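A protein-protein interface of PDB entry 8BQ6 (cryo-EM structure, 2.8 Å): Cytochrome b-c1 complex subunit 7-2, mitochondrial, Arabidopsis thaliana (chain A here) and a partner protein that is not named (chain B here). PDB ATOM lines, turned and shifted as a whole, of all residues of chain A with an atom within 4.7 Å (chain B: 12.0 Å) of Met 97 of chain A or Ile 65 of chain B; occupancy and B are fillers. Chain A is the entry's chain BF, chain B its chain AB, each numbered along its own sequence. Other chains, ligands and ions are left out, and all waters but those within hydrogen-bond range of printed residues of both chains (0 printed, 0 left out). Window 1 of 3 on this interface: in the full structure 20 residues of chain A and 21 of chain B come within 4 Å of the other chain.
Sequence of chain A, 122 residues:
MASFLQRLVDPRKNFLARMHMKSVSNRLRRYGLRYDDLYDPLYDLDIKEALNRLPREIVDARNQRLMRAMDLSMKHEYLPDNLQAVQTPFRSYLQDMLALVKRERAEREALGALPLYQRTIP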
ATOM      1  N   ALA A  50      -9.409 -38.572  10.822  1.00  0.00           N
ATOM      2  CA  ALA A  50      -8.566 -37.420  11.124  1.00  0.00           C
ATOM      3  C   ALA A  50      -7.402 -37.810  12.026  1.00  0.00           C
ATOM      4  O   ALA A  50      -6.287 -37.301  11.868  1.00  0.00           O
ATOM      5  CB  ALA A  50      -9.404 -36.317  11.770  1.00  0.00           C
ATOM      6  N   ARG A  53      -4.558 -39.488  10.215  1.00  0.00           N
ATOM      7  CA  ARG A  53      -3.780 -38.630   9.336  1.00  0.00           C
ATOM      8  C   ARG A  53      -2.805 -37.730  10.080  1.00  0.00           C
ATOM      9  O   ARG A  53      -2.070 -36.978   9.434  1.00  0.00           O
ATOM     10  CB  ARG A  53      -4.714 -37.769   8.488  1.00  0.00           C
ATOM     11  CG  ARG A  53      -5.300 -38.488   7.299  1.00  0.00           C
ATOM     12  CD  ARG A  53      -6.229 -37.580   6.530  1.00  0.00           C
ATOM     13  NE  ARG A  53      -7.112 -38.346   5.663  1.00  0.00           N
ATOM     14  CZ  ARG A  53      -7.924 -37.813   4.762  1.00  0.00           C
ATOM     15  NH1 ARG A  53      -7.997 -36.505   4.587  1.00  0.00           N
ATOM     16  NH2 ARG A  53      -8.681 -38.614   4.020  1.00  0.00           N
ATOM     17  N   LEU A  54      -2.787 -37.774  11.406  1.00  0.00           N
ATOM     18  CA  LEU A  54      -1.892 -36.921  12.167  1.00  0.00           C
ATOM     19  C   LEU A  54      -0.533 -37.588  12.344  1.00  0.00           C
ATOM     20  O   LEU A  54      -0.421 -38.816  12.306  1.00  0.00           O
ATOM     21  CB  LEU A  54      -2.504 -36.598  13.527  1.00  0.00           C
ATOM     22  CG  LEU A  54      -3.666 -35.600  13.534  1.00  0.00           C
ATOM     23  CD1 LEU A  54      -4.289 -35.509  14.916  1.00  0.00           C
ATOM     24  CD2 LEU A  54      -3.219 -34.228  13.055  1.00  0.00           C
ATOM     25  N   LEU A  94      -6.192 -31.119  16.389  1.00  0.00           N
ATOM     26  CA  LEU A  94      -7.125 -31.996  15.696  1.00  0.00           C
ATOM     27  C   LEU A  94      -8.213 -31.273  14.918  1.00  0.00           C
ATOM     28  O   LEU A  94      -8.721 -31.831  13.942  1.00  0.00           O
ATOM     29  CB  LEU A  94      -7.792 -32.943  16.704  1.00  0.00           C
ATOM     30  CG  LEU A  94      -8.784 -33.957  16.142  1.00  0.00           C
ATOM     31  CD1 LEU A  94      -8.086 -34.903  15.184  1.00  0.00           C
ATOM     32  CD2 LEU A  94      -9.450 -34.709  17.271  1.00  0.00           C
ATOM     33  N   GLN A  95      -8.585 -30.056  15.313  1.00  0.00           N
ATOM     34  CA  GLN A  95      -9.726 -29.396  14.683  1.00  0.00           C
ATOM     35  C   GLN A  95      -9.463 -29.093  13.214  1.00  0.00           C
ATOM     36  O   GLN A  95     -10.346 -29.285  12.369  1.00  0.00           O
ATOM     37  CB  GLN A  95     -10.071 -28.118  15.441  1.00  0.00           C
ATOM     38  CG  GLN A  95     -10.699 -28.369  16.796  1.00  0.00           C
ATOM     39  CD  GLN A  95     -11.920 -29.263  16.725  1.00  0.00           C
ATOM     40  OE1 GLN A  95     -12.814 -29.052  15.907  1.00  0.00           O
ATOM     41  NE2 GLN A  95     -11.962 -30.272  17.585  1.00  0.00           N
ATOM     42  N   ASP A  96      -8.261 -28.616  12.886  1.00  0.00           N
ATOM     43  CA  ASP A  96      -7.945 -28.310  11.494  1.00  0.00           C
ATOM     44  C   ASP A  96      -7.985 -29.563  10.628  1.00  0.00           C
ATOM     45  O   ASP A  96      -8.500 -29.531   9.505  1.00  0.00           O
ATOM     46  CB  ASP A  96      -6.578 -27.635  11.404  1.00  0.00           C
ATOM     47  CG  ASP A  96      -6.600 -26.207  11.912  1.00  0.00           C
ATOM     48  OD1 ASP A  96      -5.653 -25.451  11.607  1.00  0.00           O
ATOM     49  OD2 ASP A  96      -7.566 -25.838  12.611  1.00  0.00           O
ATOM     50  N   MET A  97      -7.449 -30.675  11.135  1.00  0.00           N
ATOM     51  CA  MET A  97      -7.495 -31.936  10.400  1.00  0.00           C
ATOM     52  C   MET A  97      -8.924 -32.435  10.237  1.00  0.00           C
ATOM     53  O   MET A  97      -9.291 -32.952   9.176  1.00  0.00           O
ATOM     54  CB  MET A  97      -6.646 -32.984  11.114  1.00  0.00           C
ATOM     55  CG  MET A  97      -6.522 -34.298  10.370  1.00  0.00           C
ATOM     56  SD  MET A  97      -5.008 -34.371   9.405  1.00  0.00           S
ATOM     57  CE  MET A  97      -5.621 -33.868   7.810  1.00  0.00           C
ATOM     58  N   LEU A  98      -9.738 -32.307  11.287  1.00  0.00           N
ATOM     59  CA  LEU A  98     -11.114 -32.787  11.231  1.00  0.00           C
ATOM     60  C   LEU A  98     -11.946 -31.980  10.241  1.00  0.00           C
ATOM     61  O   LEU A  98     -12.770 -32.542   9.510  1.00  0.00           O
ATOM     62  CB  LEU A  98     -11.729 -32.739  12.629  1.00  0.00           C
ATOM     63  CG  LEU A  98     -13.148 -33.262  12.852  1.00  0.00           C
ATOM     64  CD1 LEU A  98     -13.308 -34.698  12.389  1.00  0.00           C
ATOM     65  CD2 LEU A  98     -13.516 -33.133  14.315  1.00  0.00           C
ATOM     66  N   ALA A  99     -11.752 -30.660  10.202  1.00  0.00           N
ATOM     67  CA  ALA A  99     -12.462 -29.842   9.224  1.00  0.00           C
ATOM     68  C   ALA A  99     -12.047 -30.200   7.802  1.00  0.00           C
ATOM     69  O   ALA A  99     -12.866 -30.162   6.878  1.00  0.00           O
ATOM     70  CB  ALA A  99     -12.216 -28.359   9.495  1.00  0.00           C
ATOM     71  N   LEU A 100     -10.772 -30.534   7.606  1.00  0.00           N
ATOM     72  CA  LEU A 100     -10.313 -30.953   6.288  1.00  0.00           C
ATOM     73  C   LEU A 100     -10.951 -32.274   5.883  1.00  0.00           C
ATOM     74  O   LEU A 100     -11.329 -32.462   4.720  1.00  0.00           O
ATOM     75  CB  LEU A 100      -8.788 -31.053   6.282  1.00  0.00           C
ATOM     76  CG  LEU A 100      -8.085 -31.691   5.088  1.00  0.00           C
ATOM     77  CD1 LEU A 100      -6.751 -31.020   4.899  1.00  0.00           C
ATOM     78  CD2 LEU A 100      -7.879 -33.172   5.304  1.00  0.00           C
ATOM     79  N   VAL A 101     -11.068 -33.206   6.830  1.00  0.00           N
ATOM     80  CA  VAL A 101     -11.704 -34.488   6.547  1.00  0.00           C
ATOM     81  C   VAL A 101     -13.169 -34.285   6.182  1.00  0.00           C
ATOM     82  O   VAL A 101     -13.681 -34.899   5.237  1.00  0.00           O
ATOM     83  CB  VAL A 101     -11.543 -35.429   7.755  1.00  0.00           C
ATOM     84  CG1 VAL A 101     -12.553 -36.559   7.698  1.00  0.00           C
ATOM     85  CG2 VAL A 101     -10.127 -35.963   7.825  1.00  0.00           C
ATOM     86  N   HIS B  56       5.520 -28.916  18.133  1.00  0.00           N
ATOM     87  CA  HIS B  56       6.101 -28.424  16.890  1.00  0.00           C
ATOM     88  C   HIS B  56       5.601 -29.230  15.698  1.00  0.00           C
ATOM     89  O   HIS B  56       5.401 -28.683  14.607  1.00  0.00           O
ATOM     90  CB  HIS B  56       7.626 -28.463  16.982  1.00  0.00           C
ATOM     91  CG  HIS B  56       8.319 -28.280  15.669  1.00  0.00           C
ATOM     92  ND1 HIS B  56       8.380 -27.064  15.023  1.00  0.00           N
ATOM     93  CD2 HIS B  56       8.990 -29.157  14.887  1.00  0.00           C
ATOM     94  CE1 HIS B  56       9.053 -27.202  13.894  1.00  0.00           C
ATOM     95  NE2 HIS B  56       9.436 -28.461  13.789  1.00  0.00           N
ATOM     96  N   ALA B  57       5.392 -30.533  15.887  1.00  0.00           N
ATOM     97  CA  ALA B  57       4.841 -31.354  14.814  1.00  0.00           C
ATOM     98  C   ALA B  57       3.392 -30.982  14.528  1.00  0.00           C
ATOM     99  O   ALA B  57       2.960 -30.982  13.370  1.00  0.00           O
ATOM    100  CB  ALA B  57       4.962 -32.832  15.173  1.00  0.00           C
ATOM    101  N   ALA B  58       2.625 -30.663  15.572  1.00  0.00           N
ATOM    102  CA  ALA B  58       1.239 -30.254  15.371  1.00  0.00           C
ATOM    103  C   ALA B  58       1.154 -28.924  14.636  1.00  0.00           C
ATOM    104  O   ALA B  58       0.264 -28.724  13.803  1.00  0.00           O
ATOM    105  CB  ALA B  58       0.514 -30.178  16.711  1.00  0.00           C
ATOM    106  N   GLU B  59       2.064 -27.995  14.939  1.00  0.00           N
ATOM    107  CA  GLU B  59       2.062 -26.712  14.243  1.00  0.00           C
ATOM    108  C   GLU B  59       2.405 -26.884  12.768  1.00  0.00           C
ATOM    109  O   GLU B  59       1.847 -26.192  11.908  1.00  0.00           O
ATOM    110  CB  GLU B  59       3.045 -25.748  14.911  1.00  0.00           C
ATOM    111  CG  GLU B  59       2.482 -24.970  16.094  1.00  0.00           C
ATOM    112  CD  GLU B  59       1.292 -24.099  15.730  1.00  0.00           C
ATOM    113  OE1 GLU B  59       1.366 -23.361  14.724  1.00  0.00           O
ATOM    114  OE2 GLU B  59       0.280 -24.145  16.458  1.00  0.00           O
ATOM    115  N   ILE B  60       3.329 -27.797  12.458  1.00  0.00           N
ATOM    116  CA  ILE B  60       3.764 -27.995  11.076  1.00  0.00           C
ATOM    117  C   ILE B  60       2.617 -28.515  10.221  1.00  0.00           C
ATOM    118  O   ILE B  60       2.387 -28.045   9.101  1.00  0.00           O
ATOM    119  CB  ILE B  60       4.969 -28.950  11.027  1.00  0.00           C
ATOM    120  CG1 ILE B  60       6.268 -28.183  11.233  1.00  0.00           C
ATOM    121  CG2 ILE B  60       5.006 -29.724   9.712  1.00  0.00           C
ATOM    122  CD1 ILE B  60       7.461 -29.085  11.314  1.00  0.00           C
ATOM    123  N   ILE B  61       1.890 -29.510  10.730  1.00  0.00           N
ATOM    124  CA  ILE B  61       0.791 -30.075   9.960  1.00  0.00           C
ATOM    125  C   ILE B  61      -0.360 -29.084   9.858  1.00  0.00           C
ATOM    126  O   ILE B  61      -1.070 -29.044   8.847  1.00  0.00           O
ATOM    127  CB  ILE B  61       0.346 -31.422  10.564  1.00  0.00           C
ATOM    128  CG1 ILE B  61      -0.564 -32.161   9.585  1.00  0.00           C
ATOM    129  CG2 ILE B  61      -0.360 -31.228  11.892  1.00  0.00           C
ATOM    130  CD1 ILE B  61      -0.101 -32.092   8.150  1.00  0.00           C
ATOM    131  N   LYS B  62      -0.565 -28.268  10.893  1.00  0.00           N
ATOM    132  CA  LYS B  62      -1.627 -27.269  10.843  1.00  0.00           C
ATOM    133  C   LYS B  62      -1.334 -26.210   9.791  1.00  0.00           C
ATOM    134  O   LYS B  62      -2.250 -25.716   9.124  1.00  0.00           O
ATOM    135  CB  LYS B  62      -1.810 -26.620  12.212  1.00  0.00           C
ATOM    136  CG  LYS B  62      -2.622 -27.446  13.188  1.00  0.00           C
ATOM    137  CD  LYS B  62      -3.164 -26.588  14.314  1.00  0.00           C
ATOM    138  CE  LYS B  62      -2.075 -26.207  15.296  1.00  0.00           C
ATOM    139  NZ  LYS B  62      -2.620 -26.000  16.666  1.00  0.00           N
ATOM    140  N   ASN B  63      -0.060 -25.832   9.647  1.00  0.00           N
ATOM    141  CA  ASN B  63       0.317 -24.839   8.647  1.00  0.00           C
ATOM    142  C   ASN B  63       0.070 -25.357   7.237  1.00  0.00           C
ATOM    143  O   ASN B  63      -0.357 -24.602   6.357  1.00  0.00           O
ATOM    144  CB  ASN B  63       1.786 -24.454   8.815  1.00  0.00           C
ATOM    145  CG  ASN B  63       2.025 -23.566  10.013  1.00  0.00           C
ATOM    146  OD1 ASN B  63       1.102 -23.246  10.761  1.00  0.00           O
ATOM    147  ND2 ASN B  63       3.272 -23.155  10.199  1.00  0.00           N
ATOM    148  N   LYS B  64       0.357 -26.638   7.003  1.00  0.00           N
ATOM    149  CA  LYS B  64       0.101 -27.229   5.696  1.00  0.00           C
ATOM    150  C   LYS B  64      -1.390 -27.262   5.390  1.00  0.00           C
ATOM    151  O   LYS B  64      -1.803 -27.033   4.249  1.00  0.00           O
ATOM    152  CB  LYS B  64       0.693 -28.636   5.638  1.00  0.00           C
ATOM    153  CG  LYS B  64       1.083 -29.099   4.248  1.00  0.00           C
ATOM    154  CD  LYS B  64       1.390 -30.591   4.247  1.00  0.00           C
ATOM    155  CE  LYS B  64       2.423 -30.967   3.195  1.00  0.00           C
ATOM    156  NZ  LYS B  64       2.429 -30.067   2.012  1.00  0.00           N
ATOM    157  N   ILE B  65      -2.213 -27.558   6.397  1.00  0.00           N
ATOM    158  CA  ILE B  65      -3.653 -27.618   6.177  1.00  0.00           C
ATOM    159  C   ILE B  65      -4.189 -26.252   5.773  1.00  0.00           C
ATOM    160  O   ILE B  65      -5.021 -26.140   4.866  1.00  0.00           O
ATOM    161  CB  ILE B  65      -4.360 -28.156   7.432  1.00  0.00           C
ATOM    162  CG1 ILE B  65      -3.907 -29.585   7.707  1.00  0.00           C
ATOM    163  CG2 ILE B  65      -5.868 -28.121   7.244  1.00  0.00           C
ATOM    164  CD1 ILE B  65      -4.873 -30.376   8.523  1.00  0.00           C
ATOM    165  N   LYS B  66      -3.722 -25.192   6.439  1.00  0.00           N
ATOM    166  CA  LYS B  66      -4.133 -23.844   6.064  1.00  0.00           C
ATOM    167  C   LYS B  66      -3.700 -23.511   4.645  1.00  0.00           C
ATOM    168  O   LYS B  66      -4.370 -22.741   3.946  1.00  0.00           O
ATOM    169  CB  LYS B  66      -3.556 -22.827   7.046  1.00  0.00           C
ATOM    170  CG  LYS B  66      -4.091 -22.960   8.455  1.00  0.00           C
ATOM    171  CD  LYS B  66      -3.847 -21.694   9.261  1.00  0.00           C
ATOM    172  CE  LYS B  66      -2.526 -21.029   8.893  1.00  0.00           C
ATOM    173  NZ  LYS B  66      -1.439 -21.388   9.840  1.00  0.00           N
ATOM    174  N   LYS B  67      -2.576 -24.076   4.202  1.00  0.00           N
ATOM    175  CA  LYS B  67      -2.137 -23.857   2.829  1.00  0.00           C
ATOM    176  C   LYS B  67      -3.137 -24.441   1.837  1.00  0.00           C
ATOM    177  O   LYS B  67      -3.493 -23.788   0.849  1.00  0.00           O
ATOM    178  CB  LYS B  67      -0.747 -24.462   2.628  1.00  0.00           C
ATOM    179  CG  LYS B  67       0.369 -23.429   2.542  1.00  0.00           C
ATOM    180  CD  LYS B  67       1.564 -23.970   1.786  1.00  0.00           C
ATOM    181  CE  LYS B  67       1.210 -24.273   0.343  1.00  0.00           C
ATOM    182  NZ  LYS B  67       1.042 -23.030  -0.464  1.00  0.00           N
ATOM    183  N   LEU B  68      -3.623 -25.658   2.100  1.00  0.00           N
ATOM    184  CA  LEU B  68      -4.634 -26.269   1.244  1.00  0.00           C
ATOM    185  C   LEU B  68      -5.979 -25.563   1.336  1.00  0.00           C
ATOM    186  O   LEU B  68      -6.845 -25.794   0.486  1.00  0.00           O
ATOM    187  CB  LEU B  68      -4.819 -27.745   1.604  1.00  0.00           C
ATOM    188  CG  LEU B  68      -3.565 -28.605   1.749  1.00  0.00           C
ATOM    189  CD1 LEU B  68      -3.845 -29.805   2.633  1.00  0.00           C
ATOM    190  CD2 LEU B  68      -3.074 -29.052   0.385  1.00  0.00           C
ATOM    191  N   GLU B  69      -6.171 -24.715   2.348  1.00  0.00           N
ATOM    192  CA  GLU B  69      -7.464 -24.081   2.582  1.00  0.00           C
ATOM    193  C   GLU B  69      -7.759 -22.940   1.619  1.00  0.00           C
ATOM    194  O   GLU B  69      -8.926 -22.572   1.460  1.00  0.00           O
ATOM    195  CB  GLU B  69      -7.534 -23.553   4.013  1.00  0.00           C
ATOM    196  CG  GLU B  69      -7.811 -24.601   5.069  1.00  0.00           C
ATOM    197  CD  GLU B  69      -9.259 -24.608   5.496  1.00  0.00           C
ATOM    198  OE1 GLU B  69     -10.130 -24.310   4.654  1.00  0.00           O
ATOM    199  OE2 GLU B  69      -9.524 -24.880   6.684  1.00  0.00           O
ATOM    200  N   ASN B  70      -6.738 -22.361   0.992  1.00  0.00           N
ATOM    201  CA  ASN B  70      -6.910 -21.228   0.079  1.00  0.00           C
ATOM    202  C   ASN B  70      -6.515 -21.608  -1.356  1.00  0.00           C
ATOM    203  O   ASN B  70      -5.358 -21.553  -1.770  1.00  0.00           O
ATOM    204  CB  ASN B  70      -6.172 -19.977   0.593  1.00  0.00           C
ATOM    205  CG  ASN B  70      -4.722 -19.826   0.050  1.00  0.00           C
ATOM    206  OD1 ASN B  70      -4.138 -20.699  -0.512  1.00  0.00           O
ATOM    207  ND2 ASN B  70      -4.184 -18.678   0.203  1.00  0.00           N
ATOM    208  N   PRO B  71      -7.396 -22.042  -2.187  1.00  0.00           N
ATOM    209  CA  PRO B  71      -6.959 -22.460  -3.519  1.00  0.00           C
ATOM    210  C   PRO B  71      -6.631 -21.286  -4.437  1.00  0.00           C
ATOM    211  O   PRO B  71      -7.055 -20.149  -4.221  1.00  0.00           O
ATOM    212  CB  PRO B  71      -8.164 -23.237  -4.028  1.00  0.00           C
ATOM    213  CG  PRO B  71      -9.312 -22.593  -3.324  1.00  0.00           C
ATOM    214  CD  PRO B  71      -8.817 -22.208  -1.963  1.00  0.00           C
ATOM    215  N   ASP B  72      -5.879 -21.593  -5.492  1.00  0.00           N
ATOM    216  CA  ASP B  72      -5.467 -20.611  -6.486  1.00  0.00           C
ATOM    217  C   ASP B  72      -6.424 -20.667  -7.668  1.00  0.00           C
ATOM    218  O   ASP B  72      -6.614 -21.731  -8.266  1.00  0.00           O
ATOM    219  CB  ASP B  72      -4.033 -20.878  -6.943  1.00  0.00           C
ATOM    220  CG  ASP B  72      -3.411 -19.691  -7.642  1.00  0.00           C
ATOM    221  OD1 ASP B  72      -3.924 -18.564  -7.472  1.00  0.00           O
ATOM    222  OD2 ASP B  72      -2.403 -19.881  -8.354  1.00  0.00           O
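The side-chain carboxylate (OE2) of Glu 59 of chain B lies within salt-bridge range of the side-chain amino group (NZ) of Lys 62 of chain B, at 3.4 Å.
Among the printed residues, merely in contact across the chains: Met 97 of chain A with Ile 65 of chain B (3.6 Å), Asp 96 of chain A with Ile 65 of chain B (3.7 Å), Leu 100 of chain A with Ile 65 of chain B (3.8 Å), Asp 96 of chain A with Lys 62 of chain B (3.8 Å) and Leu 100 of chain A with Leu 68 of chain B (3.9 Å).
No residue of chain B comes within 4 Å of Leu 54 of chain A. Leu 94 of chain A touches none of the printed residues of chain B. No residue of chain B comes within 4 Å of Gln 95 of chain A. Of the printed residues of chain B, Asp 96 of chain A touches Lys 62 and Ile 65. Of chain B, only Ile 65 comes within 4 Å of Met 97 of chain A. Val 101 of chain A touches none of the printed residues of chain B. Printed residues of chain A within 4 Å of Lys 62 of chain B: Asp 96. Ile 65 of chain B touches just these residues of chain A: Asp 96, Met 97 and Leu 100. Printed residues of chain A within 4 Å of Leu 68 of chain B: Leu 100. The nearest printed residue of chain A that does not touch Lys 62 of chain B is Leu 94 of chain A (5.8 Å).
Of the 11 printed residues of chain A, 3 touch a printed residue of chain B. Printed residues of chain A that touch a printed residue of chain B: Asp 96, Met 97 and Leu 100. Hydrophobic or aromatic side chains of chain A within 4 Å of the printed part of chain B: Met 97 and Leu 100. Among the printed residues, 5 pairs touch across the chains. Among the printed residues, no Asp or Glu carboxylate lies within 4 Å of a Lys or Arg side-chain nitrogen of the other chain.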
